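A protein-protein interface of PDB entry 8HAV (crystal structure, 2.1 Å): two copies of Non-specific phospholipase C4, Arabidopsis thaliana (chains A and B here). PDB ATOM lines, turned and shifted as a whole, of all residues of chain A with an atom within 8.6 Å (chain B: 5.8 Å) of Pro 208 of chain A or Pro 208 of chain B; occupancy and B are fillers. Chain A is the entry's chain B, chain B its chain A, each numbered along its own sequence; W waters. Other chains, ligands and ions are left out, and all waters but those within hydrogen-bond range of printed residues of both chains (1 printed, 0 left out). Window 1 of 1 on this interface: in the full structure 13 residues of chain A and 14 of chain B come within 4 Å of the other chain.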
ATOM      1  N   GLN A 159     -11.897   4.029 -30.987  1.00  0.00           N
ATOM      2  CA  GLN A 159     -12.457   4.235 -29.648  1.00  0.00           C
ATOM      3  C   GLN A 159     -13.671   5.159 -29.584  1.00  0.00           C
ATOM      4  O   GLN A 159     -14.575   4.896 -28.776  1.00  0.00           O
ATOM      5  CB  GLN A 159     -11.377   4.679 -28.680  1.00  0.00           C
ATOM      6  CG  GLN A 159     -10.327   3.591 -28.442  1.00  0.00           C
ATOM      7  CD  GLN A 159     -10.918   2.316 -27.820  1.00  0.00           C
ATOM      8  OE1 GLN A 159     -11.982   2.334 -27.200  1.00  0.00           O
ATOM      9  NE2 GLN A 159     -10.230   1.208 -28.006  1.00  0.00           N
ATOM     10  N   LEU A 182      -7.437   6.431 -20.600  1.00  0.00           N
ATOM     11  CA  LEU A 182      -7.048   5.949 -19.275  1.00  0.00           C
ATOM     12  C   LEU A 182      -7.766   6.728 -18.180  1.00  0.00           C
ATOM     13  O   LEU A 182      -8.243   6.144 -17.197  1.00  0.00           O
ATOM     14  CB  LEU A 182      -5.521   6.058 -19.122  1.00  0.00           C
ATOM     15  CG  LEU A 182      -4.709   5.098 -20.005  1.00  0.00           C
ATOM     16  CD1 LEU A 182      -3.219   5.431 -20.020  1.00  0.00           C
ATOM     17  CD2 LEU A 182      -4.935   3.650 -19.560  1.00  0.00           C
ATOM     18  N   ILE A 203     -19.511  -8.614 -18.837  1.00  0.00           N
ATOM     19  CA  ILE A 203     -18.497  -8.304 -19.834  1.00  0.00           C
ATOM     20  C   ILE A 203     -17.453  -9.411 -19.771  1.00  0.00           C
ATOM     21  O   ILE A 203     -16.761  -9.570 -18.757  1.00  0.00           O
ATOM     22  CB  ILE A 203     -17.877  -6.920 -19.596  1.00  0.00           C
ATOM     23  CG1 ILE A 203     -18.969  -5.838 -19.699  1.00  0.00           C
ATOM     24  CG2 ILE A 203     -16.715  -6.695 -20.548  1.00  0.00           C
ATOM     25  CD1 ILE A 203     -18.598  -4.499 -19.101  1.00  0.00           C
ATOM     26  N   TYR A 205     -14.095 -10.803 -21.147  1.00  0.00           N
ATOM     27  CA  TYR A 205     -12.910 -10.249 -21.788  1.00  0.00           C
ATOM     28  C   TYR A 205     -11.759 -11.249 -21.843  1.00  0.00           C
ATOM     29  O   TYR A 205     -11.595 -12.094 -20.956  1.00  0.00           O
ATOM     30  CB  TYR A 205     -12.432  -8.997 -21.049  1.00  0.00           C
ATOM     31  CG  TYR A 205     -11.896  -9.283 -19.659  1.00  0.00           C
ATOM     32  CD1 TYR A 205     -12.756  -9.393 -18.572  1.00  0.00           C
ATOM     33  CD2 TYR A 205     -10.535  -9.458 -19.431  1.00  0.00           C
ATOM     34  CE1 TYR A 205     -12.282  -9.668 -17.304  1.00  0.00           C
ATOM     35  CE2 TYR A 205     -10.044  -9.726 -18.155  1.00  0.00           C
ATOM     36  CZ  TYR A 205     -10.923  -9.829 -17.099  1.00  0.00           C
ATOM     37  OH  TYR A 205     -10.455 -10.098 -15.829  1.00  0.00           O
ATOM     38  N   GLN A 206     -10.939 -11.121 -22.889  1.00  0.00           N
ATOM     39  CA  GLN A 206      -9.733 -11.931 -23.034  1.00  0.00           C
ATOM     40  C   GLN A 206      -8.518 -11.135 -22.567  1.00  0.00           C
ATOM     41  O   GLN A 206      -7.869 -11.494 -21.576  1.00  0.00           O
ATOM     42  CB  GLN A 206      -9.565 -12.382 -24.487  1.00  0.00           C
ATOM     43  CG  GLN A 206     -10.080 -13.799 -24.776  1.00  0.00           C
ATOM     44  CD  GLN A 206     -10.740 -13.931 -26.155  1.00  0.00           C
ATOM     45  OE1 GLN A 206     -10.998 -12.933 -26.825  1.00  0.00           O
ATOM     46  NE2 GLN A 206     -11.042 -15.163 -26.562  1.00  0.00           N
ATOM     47  N   PHE A 207      -8.173 -10.096 -23.319  1.00  0.00           N
ATOM     48  CA  PHE A 207      -7.131  -9.155 -22.955  1.00  0.00           C
ATOM     49  C   PHE A 207      -7.834  -7.963 -22.275  1.00  0.00           C
ATOM     50  O   PHE A 207      -9.062  -8.024 -22.083  1.00  0.00           O
ATOM     51  CB  PHE A 207      -6.312  -8.763 -24.191  1.00  0.00           C
ATOM     52  CG  PHE A 207      -5.555  -9.933 -24.832  1.00  0.00           C
ATOM     53  CD1 PHE A 207      -6.183 -10.760 -25.752  1.00  0.00           C
ATOM     54  CD2 PHE A 207      -4.222 -10.176 -24.521  1.00  0.00           C
ATOM     55  CE1 PHE A 207      -5.499 -11.818 -26.351  1.00  0.00           C
ATOM     56  CE2 PHE A 207      -3.532 -11.240 -25.123  1.00  0.00           C
ATOM     57  CZ  PHE A 207      -4.177 -12.059 -26.035  1.00  0.00           C
ATOM     58  N   PRO A 208      -7.134  -6.888 -21.860  1.00  0.00           N
ATOM     59  CA  PRO A 208      -7.828  -5.742 -21.199  1.00  0.00           C
ATOM     60  C   PRO A 208      -8.899  -5.148 -22.098  1.00  0.00           C
ATOM     61  O   PRO A 208      -8.644  -4.825 -23.264  1.00  0.00           O
ATOM     62  CB  PRO A 208      -6.701  -4.729 -20.923  1.00  0.00           C
ATOM     63  CG  PRO A 208      -5.445  -5.348 -21.363  1.00  0.00           C
ATOM     64  CD  PRO A 208      -5.663  -6.736 -21.858  1.00  0.00           C
ATOM     65  N   PRO A 209     -10.131  -5.039 -21.608  1.00  0.00           N
ATOM     66  CA  PRO A 209     -11.243  -4.607 -22.465  1.00  0.00           C
ATOM     67  C   PRO A 209     -11.332  -3.098 -22.609  1.00  0.00           C
ATOM     68  O   PRO A 209     -11.044  -2.340 -21.680  1.00  0.00           O
ATOM     69  CB  PRO A 209     -12.479  -5.134 -21.722  1.00  0.00           C
ATOM     70  CG  PRO A 209     -12.065  -5.082 -20.274  1.00  0.00           C
ATOM     71  CD  PRO A 209     -10.585  -5.403 -20.249  1.00  0.00           C
ATOM     72  N   SER A 210     -11.806  -2.675 -23.780  1.00  0.00           N
ATOM     73  CA  SER A 210     -12.040  -1.261 -24.048  1.00  0.00           C
ATOM     74  C   SER A 210     -13.160  -0.683 -23.195  1.00  0.00           C
ATOM     75  O   SER A 210     -13.226   0.538 -23.014  1.00  0.00           O
ATOM     76  CB  SER A 210     -12.350  -1.067 -25.540  1.00  0.00           C
ATOM     77  OG  SER A 210     -11.151  -1.068 -26.302  1.00  0.00           O
ATOM     78  N   THR A 211     -14.050  -1.525 -22.672  1.00  0.00           N
ATOM     79  CA  THR A 211     -15.102  -1.036 -21.778  1.00  0.00           C
ATOM     80  C   THR A 211     -14.551  -0.450 -20.491  1.00  0.00           C
ATOM     81  O   THR A 211     -15.283   0.254 -19.796  1.00  0.00           O
ATOM     82  CB  THR A 211     -16.096  -2.160 -21.479  1.00  0.00           C
ATOM     83  OG1 THR A 211     -15.394  -3.397 -21.401  1.00  0.00           O
ATOM     84  CG2 THR A 211     -17.139  -2.259 -22.607  1.00  0.00           C
ATOM     85  N   LEU A 212     -13.296  -0.742 -20.145  1.00  0.00           N
ATOM     86  CA  LEU A 212     -12.668  -0.104 -18.985  1.00  0.00           C
ATOM     87  C   LEU A 212     -12.477   1.388 -19.200  1.00  0.00           C
ATOM     88  O   LEU A 212     -12.209   2.112 -18.241  1.00  0.00           O
ATOM     89  CB  LEU A 212     -11.308  -0.744 -18.687  1.00  0.00           C
ATOM     90  CG  LEU A 212     -11.012  -1.259 -17.278  1.00  0.00           C
ATOM     91  CD1 LEU A 212     -12.270  -1.755 -16.594  1.00  0.00           C
ATOM     92  CD2 LEU A 212      -9.979  -2.380 -17.346  1.00  0.00           C
ATOM     93  N   PHE A 213     -12.534   1.846 -20.451  1.00  0.00           N
ATOM     94  CA  PHE A 213     -12.475   3.272 -20.740  1.00  0.00           C
ATOM     95  C   PHE A 213     -13.731   4.009 -20.288  1.00  0.00           C
ATOM     96  O   PHE A 213     -13.749   5.247 -20.346  1.00  0.00           O
ATOM     97  CB  PHE A 213     -12.141   3.502 -22.211  1.00  0.00           C
ATOM     98  CG  PHE A 213     -10.860   2.824 -22.626  1.00  0.00           C
ATOM     99  CD1 PHE A 213      -9.817   2.678 -21.714  1.00  0.00           C
ATOM    100  CD2 PHE A 213     -10.709   2.302 -23.898  1.00  0.00           C
ATOM    101  CE1 PHE A 213      -8.647   2.036 -22.077  1.00  0.00           C
ATOM    102  CE2 PHE A 213      -9.531   1.675 -24.262  1.00  0.00           C
ATOM    103  CZ  PHE A 213      -8.509   1.537 -23.346  1.00  0.00           C
ATOM    104  N   PHE A 226     -17.192  -7.930 -14.774  1.00  0.00           N
ATOM    105  CA  PHE A 226     -16.209  -8.363 -15.747  1.00  0.00           C
ATOM    106  C   PHE A 226     -15.792  -9.793 -15.427  1.00  0.00           C
ATOM    107  O   PHE A 226     -15.536 -10.130 -14.268  1.00  0.00           O
ATOM    108  CB  PHE A 226     -14.978  -7.450 -15.732  1.00  0.00           C
ATOM    109  CG  PHE A 226     -15.224  -6.070 -16.273  1.00  0.00           C
ATOM    110  CD1 PHE A 226     -15.847  -5.106 -15.503  1.00  0.00           C
ATOM    111  CD2 PHE A 226     -14.812  -5.733 -17.555  1.00  0.00           C
ATOM    112  CE1 PHE A 226     -16.062  -3.825 -16.002  1.00  0.00           C
ATOM    113  CE2 PHE A 226     -15.017  -4.468 -18.058  1.00  0.00           C
ATOM    114  CZ  PHE A 226     -15.646  -3.508 -17.290  1.00  0.00           C
ATOM    115  N   GLU A 249     -15.566  -9.210 -25.342  1.00  0.00           N
ATOM    116  CA  GLU A 249     -14.435  -8.349 -25.662  1.00  0.00           C
ATOM    117  C   GLU A 249     -13.223  -9.225 -25.925  1.00  0.00           C
ATOM    118  O   GLU A 249     -12.799  -9.976 -25.043  1.00  0.00           O
ATOM    119  CB  GLU A 249     -14.155  -7.397 -24.501  1.00  0.00           C
ATOM    120  CG  GLU A 249     -15.196  -6.322 -24.329  1.00  0.00           C
ATOM    121  CD  GLU A 249     -14.685  -4.971 -24.748  1.00  0.00           C
ATOM    122  OE1 GLU A 249     -14.018  -4.873 -25.798  1.00  0.00           O
ATOM    123  OE2 GLU A 249     -14.938  -4.005 -24.008  1.00  0.00           O
ATOM    124  N   GLN A 250     -12.626  -9.089 -27.102  1.00  0.00           N
ATOM    125  CA  GLN A 250     -11.614 -10.045 -27.530  1.00  0.00           C
ATOM    126  C   GLN A 250     -10.213  -9.465 -27.653  1.00  0.00           C
ATOM    127  O   GLN A 250      -9.251 -10.111 -27.228  1.00  0.00           O
ATOM    128  CB  GLN A 250     -12.031 -10.690 -28.862  1.00  0.00           C
ATOM    129  CG  GLN A 250     -11.861  -9.831 -30.128  1.00  0.00           C
ATOM    130  CD  GLN A 250     -13.003  -8.840 -30.386  1.00  0.00           C
ATOM    131  OE1 GLN A 250     -13.938  -8.701 -29.587  1.00  0.00           O
ATOM    132  NE2 GLN A 250     -12.932  -8.159 -31.529  1.00  0.00           N
ATOM    133  N   ARG A 251     -10.050  -8.267 -28.194  1.00  0.00           N
ATOM    134  CA  ARG A 251      -8.723  -7.731 -28.450  1.00  0.00           C
ATOM    135  C   ARG A 251      -8.393  -6.626 -27.457  1.00  0.00           C
ATOM    136  O   ARG A 251      -9.277  -5.911 -26.979  1.00  0.00           O
ATOM    137  CB  ARG A 251      -8.616  -7.179 -29.878  1.00  0.00           C
ATOM    138  CG  ARG A 251      -8.908  -8.196 -30.968  1.00  0.00           C
ATOM    139  CD  ARG A 251      -7.706  -9.083 -31.237  1.00  0.00           C
ATOM    140  NE  ARG A 251      -7.720  -9.601 -32.599  1.00  0.00           N
ATOM    141  CZ  ARG A 251      -7.347  -8.906 -33.666  1.00  0.00           C
ATOM    142  NH1 ARG A 251      -6.897  -7.664 -33.560  1.00  0.00           N
ATOM    143  NH2 ARG A 251      -7.429  -9.471 -34.870  1.00  0.00           N
ATOM    144  N   TRP A 252      -7.107  -6.487 -27.155  1.00  0.00           N
ATOM    145  CA  TRP A 252      -6.630  -5.324 -26.423  1.00  0.00           C
ATOM    146  C   TRP A 252      -6.238  -4.250 -27.426  1.00  0.00           C
ATOM    147  O   TRP A 252      -5.551  -4.531 -28.414  1.00  0.00           O
ATOM    148  CB  TRP A 252      -5.446  -5.672 -25.518  1.00  0.00           C
ATOM    149  CG  TRP A 252      -4.171  -6.066 -26.227  1.00  0.00           C
ATOM    150  CD1 TRP A 252      -3.930  -7.234 -26.900  1.00  0.00           C
ATOM    151  CD2 TRP A 252      -2.955  -5.298 -26.305  1.00  0.00           C
ATOM    152  NE1 TRP A 252      -2.647  -7.234 -27.399  1.00  0.00           N
ATOM    153  CE2 TRP A 252      -2.028  -6.060 -27.051  1.00  0.00           C
ATOM    154  CE3 TRP A 252      -2.566  -4.036 -25.828  1.00  0.00           C
ATOM    155  CZ2 TRP A 252      -0.735  -5.605 -27.325  1.00  0.00           C
ATOM    156  CZ3 TRP A 252      -1.279  -3.585 -26.096  1.00  0.00           C
ATOM    157  CH2 TRP A 252      -0.379  -4.368 -26.841  1.00  0.00           C
ATOM    158  N   PHE A 253      -6.713  -3.033 -27.196  1.00  0.00           N
ATOM    159  CA  PHE A 253      -6.354  -1.917 -28.057  1.00  0.00           C
ATOM    160  C   PHE A 253      -5.011  -1.359 -27.590  1.00  0.00           C
ATOM    161  O   PHE A 253      -4.877  -0.955 -26.429  1.00  0.00           O
ATOM    162  CB  PHE A 253      -7.445  -0.842 -28.019  1.00  0.00           C
ATOM    163  CG  PHE A 253      -7.053   0.429 -28.711  1.00  0.00           C
ATOM    164  CD1 PHE A 253      -7.157   0.541 -30.091  1.00  0.00           C
ATOM    165  CD2 PHE A 253      -6.569   1.507 -27.986  1.00  0.00           C
ATOM    166  CE1 PHE A 253      -6.781   1.714 -30.747  1.00  0.00           C
ATOM    167  CE2 PHE A 253      -6.184   2.681 -28.627  1.00  0.00           C
ATOM    168  CZ  PHE A 253      -6.288   2.782 -30.014  1.00  0.00           C
ATOM    169  N   ASP A 254      -4.012  -1.359 -28.471  1.00  0.00           N
ATOM    170  CA  ASP A 254      -2.695  -0.826 -28.107  1.00  0.00           C
ATOM    171  C   ASP A 254      -2.765   0.696 -28.053  1.00  0.00           C
ATOM    172  O   ASP A 254      -2.545   1.387 -29.059  1.00  0.00           O
ATOM    173  CB  ASP A 254      -1.607  -1.287 -29.073  1.00  0.00           C
ATOM    174  CG  ASP A 254      -0.197  -0.958 -28.568  1.00  0.00           C
ATOM    175  OD1 ASP A 254      -0.084  -0.164 -27.616  1.00  0.00           O
ATOM    176  OD2 ASP A 254       0.799  -1.471 -29.118  1.00  0.00           O
ATOM    177  N   LEU A 255      -3.001   1.209 -26.843  1.00  0.00           N
ATOM    178  CA  LEU A 255      -3.058   2.641 -26.572  1.00  0.00           C
ATOM    179  C   LEU A 255      -1.794   3.373 -26.998  1.00  0.00           C
ATOM    180  O   LEU A 255      -1.838   4.591 -27.191  1.00  0.00           O
ATOM    181  CB  LEU A 255      -3.264   2.875 -25.076  1.00  0.00           C
ATOM    182  CG  LEU A 255      -4.604   2.588 -24.420  1.00  0.00           C
ATOM    183  CD1 LEU A 255      -4.588   3.191 -23.044  1.00  0.00           C
ATOM    184  CD2 LEU A 255      -5.725   3.204 -25.217  1.00  0.00           C
ATOM    185  N   LEU A 256      -0.668   2.667 -27.111  1.00  0.00           N
ATOM    186  CA  LEU A 256       0.624   3.273 -27.412  1.00  0.00           C
ATOM    187  C   LEU A 256       0.946   3.320 -28.903  1.00  0.00           C
ATOM    188  O   LEU A 256       2.025   3.794 -29.272  1.00  0.00           O
ATOM    189  CB  LEU A 256       1.729   2.518 -26.672  1.00  0.00           C
ATOM    190  CG  LEU A 256       1.576   2.603 -25.157  1.00  0.00           C
ATOM    191  CD1 LEU A 256       2.510   1.636 -24.437  1.00  0.00           C
ATOM    192  CD2 LEU A 256       1.803   4.032 -24.704  1.00  0.00           C
ATOM    193  N   TYR B 205       7.649  -2.857 -24.224  1.00  0.00           N
ATOM    194  CA  TYR B 205       6.491  -3.543 -23.670  1.00  0.00           C
ATOM    195  C   TYR B 205       5.945  -4.597 -24.625  1.00  0.00           C
ATOM    196  O   TYR B 205       6.007  -4.444 -25.846  1.00  0.00           O
ATOM    197  CB  TYR B 205       5.386  -2.541 -23.348  1.00  0.00           C
ATOM    198  CG  TYR B 205       4.777  -1.909 -24.583  1.00  0.00           C
ATOM    199  CD1 TYR B 205       5.387  -0.829 -25.203  1.00  0.00           C
ATOM    200  CD2 TYR B 205       3.588  -2.396 -25.127  1.00  0.00           C
ATOM    201  CE1 TYR B 205       4.837  -0.244 -26.332  1.00  0.00           C
ATOM    202  CE2 TYR B 205       3.023  -1.815 -26.255  1.00  0.00           C
ATOM    203  CZ  TYR B 205       3.656  -0.738 -26.854  1.00  0.00           C
ATOM    204  OH  TYR B 205       3.114  -0.152 -27.977  1.00  0.00           O
ATOM    205  N   GLN B 206       5.378  -5.659 -24.055  1.00  0.00           N
ATOM    206  CA  GLN B 206       4.675  -6.643 -24.866  1.00  0.00           C
ATOM    207  C   GLN B 206       3.184  -6.340 -24.827  1.00  0.00           C
ATOM    208  O   GLN B 206       2.595  -5.889 -25.816  1.00  0.00           O
ATOM    209  CB  GLN B 206       4.944  -8.069 -24.375  1.00  0.00           C
ATOM    210  CG  GLN B 206       6.180  -8.732 -24.983  1.00  0.00           C
ATOM    211  CD  GLN B 206       6.814  -9.792 -24.075  1.00  0.00           C
ATOM    212  OE1 GLN B 206       6.172 -10.318 -23.164  1.00  0.00           O
ATOM    213  NE2 GLN B 206       8.087 -10.097 -24.319  1.00  0.00           N
ATOM    214  N   PHE B 207       2.581  -6.556 -23.674  1.00  0.00           N
ATOM    215  CA  PHE B 207       1.183  -6.263 -23.404  1.00  0.00           C
ATOM    216  C   PHE B 207       1.089  -4.871 -22.781  1.00  0.00           C
ATOM    217  O   PHE B 207       2.131  -4.203 -22.660  1.00  0.00           O
ATOM    218  CB  PHE B 207       0.629  -7.370 -22.506  1.00  0.00           C
ATOM    219  CG  PHE B 207       0.709  -8.742 -23.115  1.00  0.00           C
ATOM    220  CD1 PHE B 207       1.816  -9.552 -22.905  1.00  0.00           C
ATOM    221  CD2 PHE B 207      -0.323  -9.216 -23.906  1.00  0.00           C
ATOM    222  CE1 PHE B 207       1.885 -10.817 -23.469  1.00  0.00           C
ATOM    223  CE2 PHE B 207      -0.260 -10.473 -24.472  1.00  0.00           C
ATOM    224  CZ  PHE B 207       0.846 -11.277 -24.252  1.00  0.00           C
ATOM    225  N   PRO B 208      -0.091  -4.370 -22.392  1.00  0.00           N
ATOM    226  CA  PRO B 208      -0.140  -3.028 -21.775  1.00  0.00           C
ATOM    227  C   PRO B 208       0.736  -2.972 -20.534  1.00  0.00           C
ATOM    228  O   PRO B 208       0.558  -3.761 -19.590  1.00  0.00           O
ATOM    229  CB  PRO B 208      -1.623  -2.843 -21.425  1.00  0.00           C
ATOM    230  CG  PRO B 208      -2.339  -3.753 -22.352  1.00  0.00           C
ATOM    231  CD  PRO B 208      -1.444  -4.912 -22.609  1.00  0.00           C
ATOM    232  N   PRO B 209       1.700  -2.056 -20.492  1.00  0.00           N
ATOM    233  CA  PRO B 209       2.667  -2.075 -19.395  1.00  0.00           C
ATOM    234  C   PRO B 209       2.134  -1.396 -18.152  1.00  0.00           C
ATOM    235  O   PRO B 209       1.378  -0.427 -18.209  1.00  0.00           O
ATOM    236  CB  PRO B 209       3.865  -1.324 -19.983  1.00  0.00           C
ATOM    237  CG  PRO B 209       3.229  -0.316 -20.892  1.00  0.00           C
ATOM    238  CD  PRO B 209       1.971  -0.967 -21.450  1.00  0.00           C
ATOM    239  N   SER B 210       2.587  -1.910 -17.005  1.00  0.00           N
ATOM    240  CA  SER B 210       2.233  -1.304 -15.724  1.00  0.00           C
ATOM    241  C   SER B 210       2.792   0.098 -15.596  1.00  0.00           C
ATOM    242  O   SER B 210       2.264   0.893 -14.811  1.00  0.00           O
ATOM    243  CB  SER B 210       2.739  -2.154 -14.559  1.00  0.00           C
ATOM    244  OG  SER B 210       1.880  -3.251 -14.315  1.00  0.00           O
ATOM    245  N   LEU B 212       2.360   2.401 -17.528  1.00  0.00           N
ATOM    246  CA  LEU B 212       1.313   3.344 -17.924  1.00  0.00           C
ATOM    247  C   LEU B 212       0.528   3.870 -16.720  1.00  0.00           C
ATOM    248  O   LEU B 212      -0.203   4.855 -16.849  1.00  0.00           O
ATOM    249  CB  LEU B 212       0.359   2.676 -18.913  1.00  0.00           C
ATOM    250  CG  LEU B 212       0.620   2.861 -20.407  1.00  0.00           C
ATOM    251  CD1 LEU B 212      -0.658   2.639 -21.188  1.00  0.00           C
ATOM    252  CD2 LEU B 212       1.163   4.246 -20.703  1.00  0.00           C
ATOM    253  N   ARG B 251       4.389  -8.713 -19.025  1.00  0.00           N
ATOM    254  CA  ARG B 251       3.043  -9.203 -18.776  1.00  0.00           C
ATOM    255  C   ARG B 251       2.075  -8.042 -18.607  1.00  0.00           C
ATOM    256  O   ARG B 251       2.457  -6.947 -18.193  1.00  0.00           O
ATOM    257  CB  ARG B 251       2.992 -10.091 -17.532  1.00  0.00           C
ATOM    258  CG  ARG B 251       3.929 -11.283 -17.573  1.00  0.00           C
ATOM    259  CD  ARG B 251       3.349 -12.447 -18.354  1.00  0.00           C
ATOM    260  NE  ARG B 251       3.982 -13.700 -17.960  1.00  0.00           N
ATOM    261  CZ  ARG B 251       3.656 -14.401 -16.882  1.00  0.00           C
ATOM    262  NH1 ARG B 251       2.676 -14.014 -16.076  1.00  0.00           N
ATOM    263  NH2 ARG B 251       4.331 -15.515 -16.602  1.00  0.00           N
ATOM    264  N   TRP B 252       0.819  -8.286 -18.958  1.00  0.00           N
ATOM    265  CA  TRP B 252      -0.243  -7.346 -18.634  1.00  0.00           C
ATOM    266  C   TRP B 252      -0.828  -7.725 -17.286  1.00  0.00           C
ATOM    267  O   TRP B 252      -1.106  -8.900 -17.024  1.00  0.00           O
ATOM    268  CB  TRP B 252      -1.330  -7.323 -19.710  1.00  0.00           C
ATOM    269  CG  TRP B 252      -2.114  -8.586 -19.869  1.00  0.00           C
ATOM    270  CD1 TRP B 252      -1.685  -9.760 -20.429  1.00  0.00           C
ATOM    271  CD2 TRP B 252      -3.486  -8.795 -19.499  1.00  0.00           C
ATOM    272  NE1 TRP B 252      -2.701 -10.690 -20.413  1.00  0.00           N
ATOM    273  CE2 TRP B 252      -3.816 -10.123 -19.849  1.00  0.00           C
ATOM    274  CE3 TRP B 252      -4.464  -7.989 -18.896  1.00  0.00           C
ATOM    275  CZ2 TRP B 252      -5.085 -10.662 -19.619  1.00  0.00           C
ATOM    276  CZ3 TRP B 252      -5.724  -8.526 -18.671  1.00  0.00           C
ATOM    277  CH2 TRP B 252      -6.022  -9.851 -19.031  1.00  0.00           C
ATOM    278  N   PHE B 253      -0.978  -6.737 -16.419  1.00  0.00           N
ATOM    279  CA  PHE B 253      -1.551  -6.996 -15.110  1.00  0.00           C
ATOM    280  C   PHE B 253      -3.073  -6.999 -15.235  1.00  0.00           C
ATOM    281  O   PHE B 253      -3.661  -6.005 -15.675  1.00  0.00           O
ATOM    282  CB  PHE B 253      -1.067  -5.948 -14.110  1.00  0.00           C
ATOM    283  CG  PHE B 253      -1.813  -5.969 -12.820  1.00  0.00           C
ATOM    284  CD1 PHE B 253      -1.551  -6.951 -11.873  1.00  0.00           C
ATOM    285  CD2 PHE B 253      -2.794  -5.019 -12.556  1.00  0.00           C
ATOM    286  CE1 PHE B 253      -2.253  -6.985 -10.679  1.00  0.00           C
ATOM    287  CE2 PHE B 253      -3.504  -5.050 -11.364  1.00  0.00           C
ATOM    288  CZ  PHE B 253      -3.238  -6.036 -10.433  1.00  0.00           C
ATOM    289  N   LEU B 256      -8.747  -6.473 -13.597  1.00  0.00           N
ATOM    290  CA  LEU B 256     -10.084  -6.942 -13.258  1.00  0.00           C
ATOM    291  C   LEU B 256     -10.087  -8.181 -12.370  1.00  0.00           C
ATOM    292  O   LEU B 256     -11.168  -8.650 -12.004  1.00  0.00           O
ATOM    293  CB  LEU B 256     -10.880  -7.224 -14.542  1.00  0.00           C
ATOM    294  CG  LEU B 256     -11.014  -6.005 -15.458  1.00  0.00           C
ATOM    295  CD1 LEU B 256     -11.467  -6.393 -16.837  1.00  0.00           C
ATOM    296  CD2 LEU B 256     -11.976  -5.010 -14.858  1.00  0.00           C
HETATM  297  O   HOH W   1     -13.807  -9.346 -11.337  1.00  0.00           O
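Tyr 205 of chain A touches Leu 256 of chain B, and with the chains exchanged Leu 256 of chain A touches Tyr 205 of chain B. Gln 206 of chain A touches Trp 252 of chain B, and with the chains exchanged Trp 252 of chain A touches Gln 206 of chain B. Pro 208 of chain A touches Trp 252 of chain B, and with the chains exchanged Trp 252 of chain A touches Pro 208 of chain B. Pro 209 of chain A touches Leu 256 of chain B, and with the chains exchanged Leu 256 of chain A touches Pro 209 of chain B.
Printed residues of chain B that touch a printed residue of chain A: Tyr 205, Gln 206, Phe 207, Pro 208, Pro 209, Leu 212, Trp 252 and Leu 256. Along chain B the printed residues that touch a printed residue of chain A span positions 205 to 256. Hydrophobic or aromatic side chains of chain A that line the printed part of chain B: Leu 182, Tyr 205, Phe 207, Pro 208, Pro 209, Leu 212, Phe 226, Trp 252 and Leu 256. Along chain A the printed residues that touch a printed residue of chain B span positions 182 to 256. Among the printed residues, 14 pairs touch across the chains.
Among the printed residues, merely in contact across the chains: Tyr 205 of chain A with Leu 256 of chain B (3.2 Å), Leu 256 of chain A with Tyr 205 of chain B (3.3 Å), Phe 207 of chain A with Phe 207 of chain B (3.4 Å), Pro 208 of chain A with Trp 252 of chain B (3.4 Å), Phe 226 of chain A with Leu 256 of chain B (3.5 Å), Trp 252 of chain A with Gln 206 of chain B (3.5 Å), Trp 252 of chain A with Pro 208 of chain B (3.5 Å), Gln 206 of chain A with Trp 252 of chain B (3.5 Å), Pro 208 of chain A with Pro 208 of chain B (3.6 Å), Pro 209 of chain A with Leu 256 of chain B (3.7 Å), Leu 212 of chain A with Leu 256 of chain B (3.7 Å), Leu 182 of chain A with Leu 212 of chain B (3.96 Å) and Leu 256 of chain A with Pro 209 of chain B (3.999 Å).
Water W1 bridges the backbone carbonyl oxygen (O) of Leu 256 of chain B and the backbone carbonyl oxygen (O) of Phe 226 of chain A.
Ile 203 of chain A touches none of the printed residues of chain B. Printed residues of chain B within 4 Å of Gln 206 of chain A: Trp 252. Of chain B, only Pro 208 and Trp 252 come within 4 Å of Pro 208 of chain A. Of the printed residues of chain B, Pro 209 of chain A touches Leu 256 (3.7 Å). Of the printed residues of chain B, Trp 252 of chain A touches Gln 206 (3.5 Å) and Pro 208 (3.5 Å). Of the printed residues of chain B, Asp 254 of chain A touches Tyr 205. Of the printed residues of chain A, Phe 207 of chain B touches Phe 207 (3.4 Å). Pro 208 of chain B touches two residues of chain A. Phe 253 of chain B touches none of the printed residues of chain A. The nearest printed residue of chain B that does not touch Leu 212 of chain A is Phe 253 of chain B (7.5 Å).
The backbone NH of Gln 206 of chain A sits at hydrogen-bond distance from the backbone carbonyl oxygen of Glu 249 of chain A, 3.1 Å away. The backbone NH of Leu 256 of chain A is in hydrogen-bond range of the side-chain carboxylate of Asp 254 of chain A, at 2.9 Å. OE1 of Gln 206 of chain A sits close to O of Gln 250 of chain A (3.3 Å).
The side-chain carboxylate of Asp 254 of chain A sits at hydrogen-bond distance from the side-chain hydroxyl of Tyr 205 of chain B (2.9 Å).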
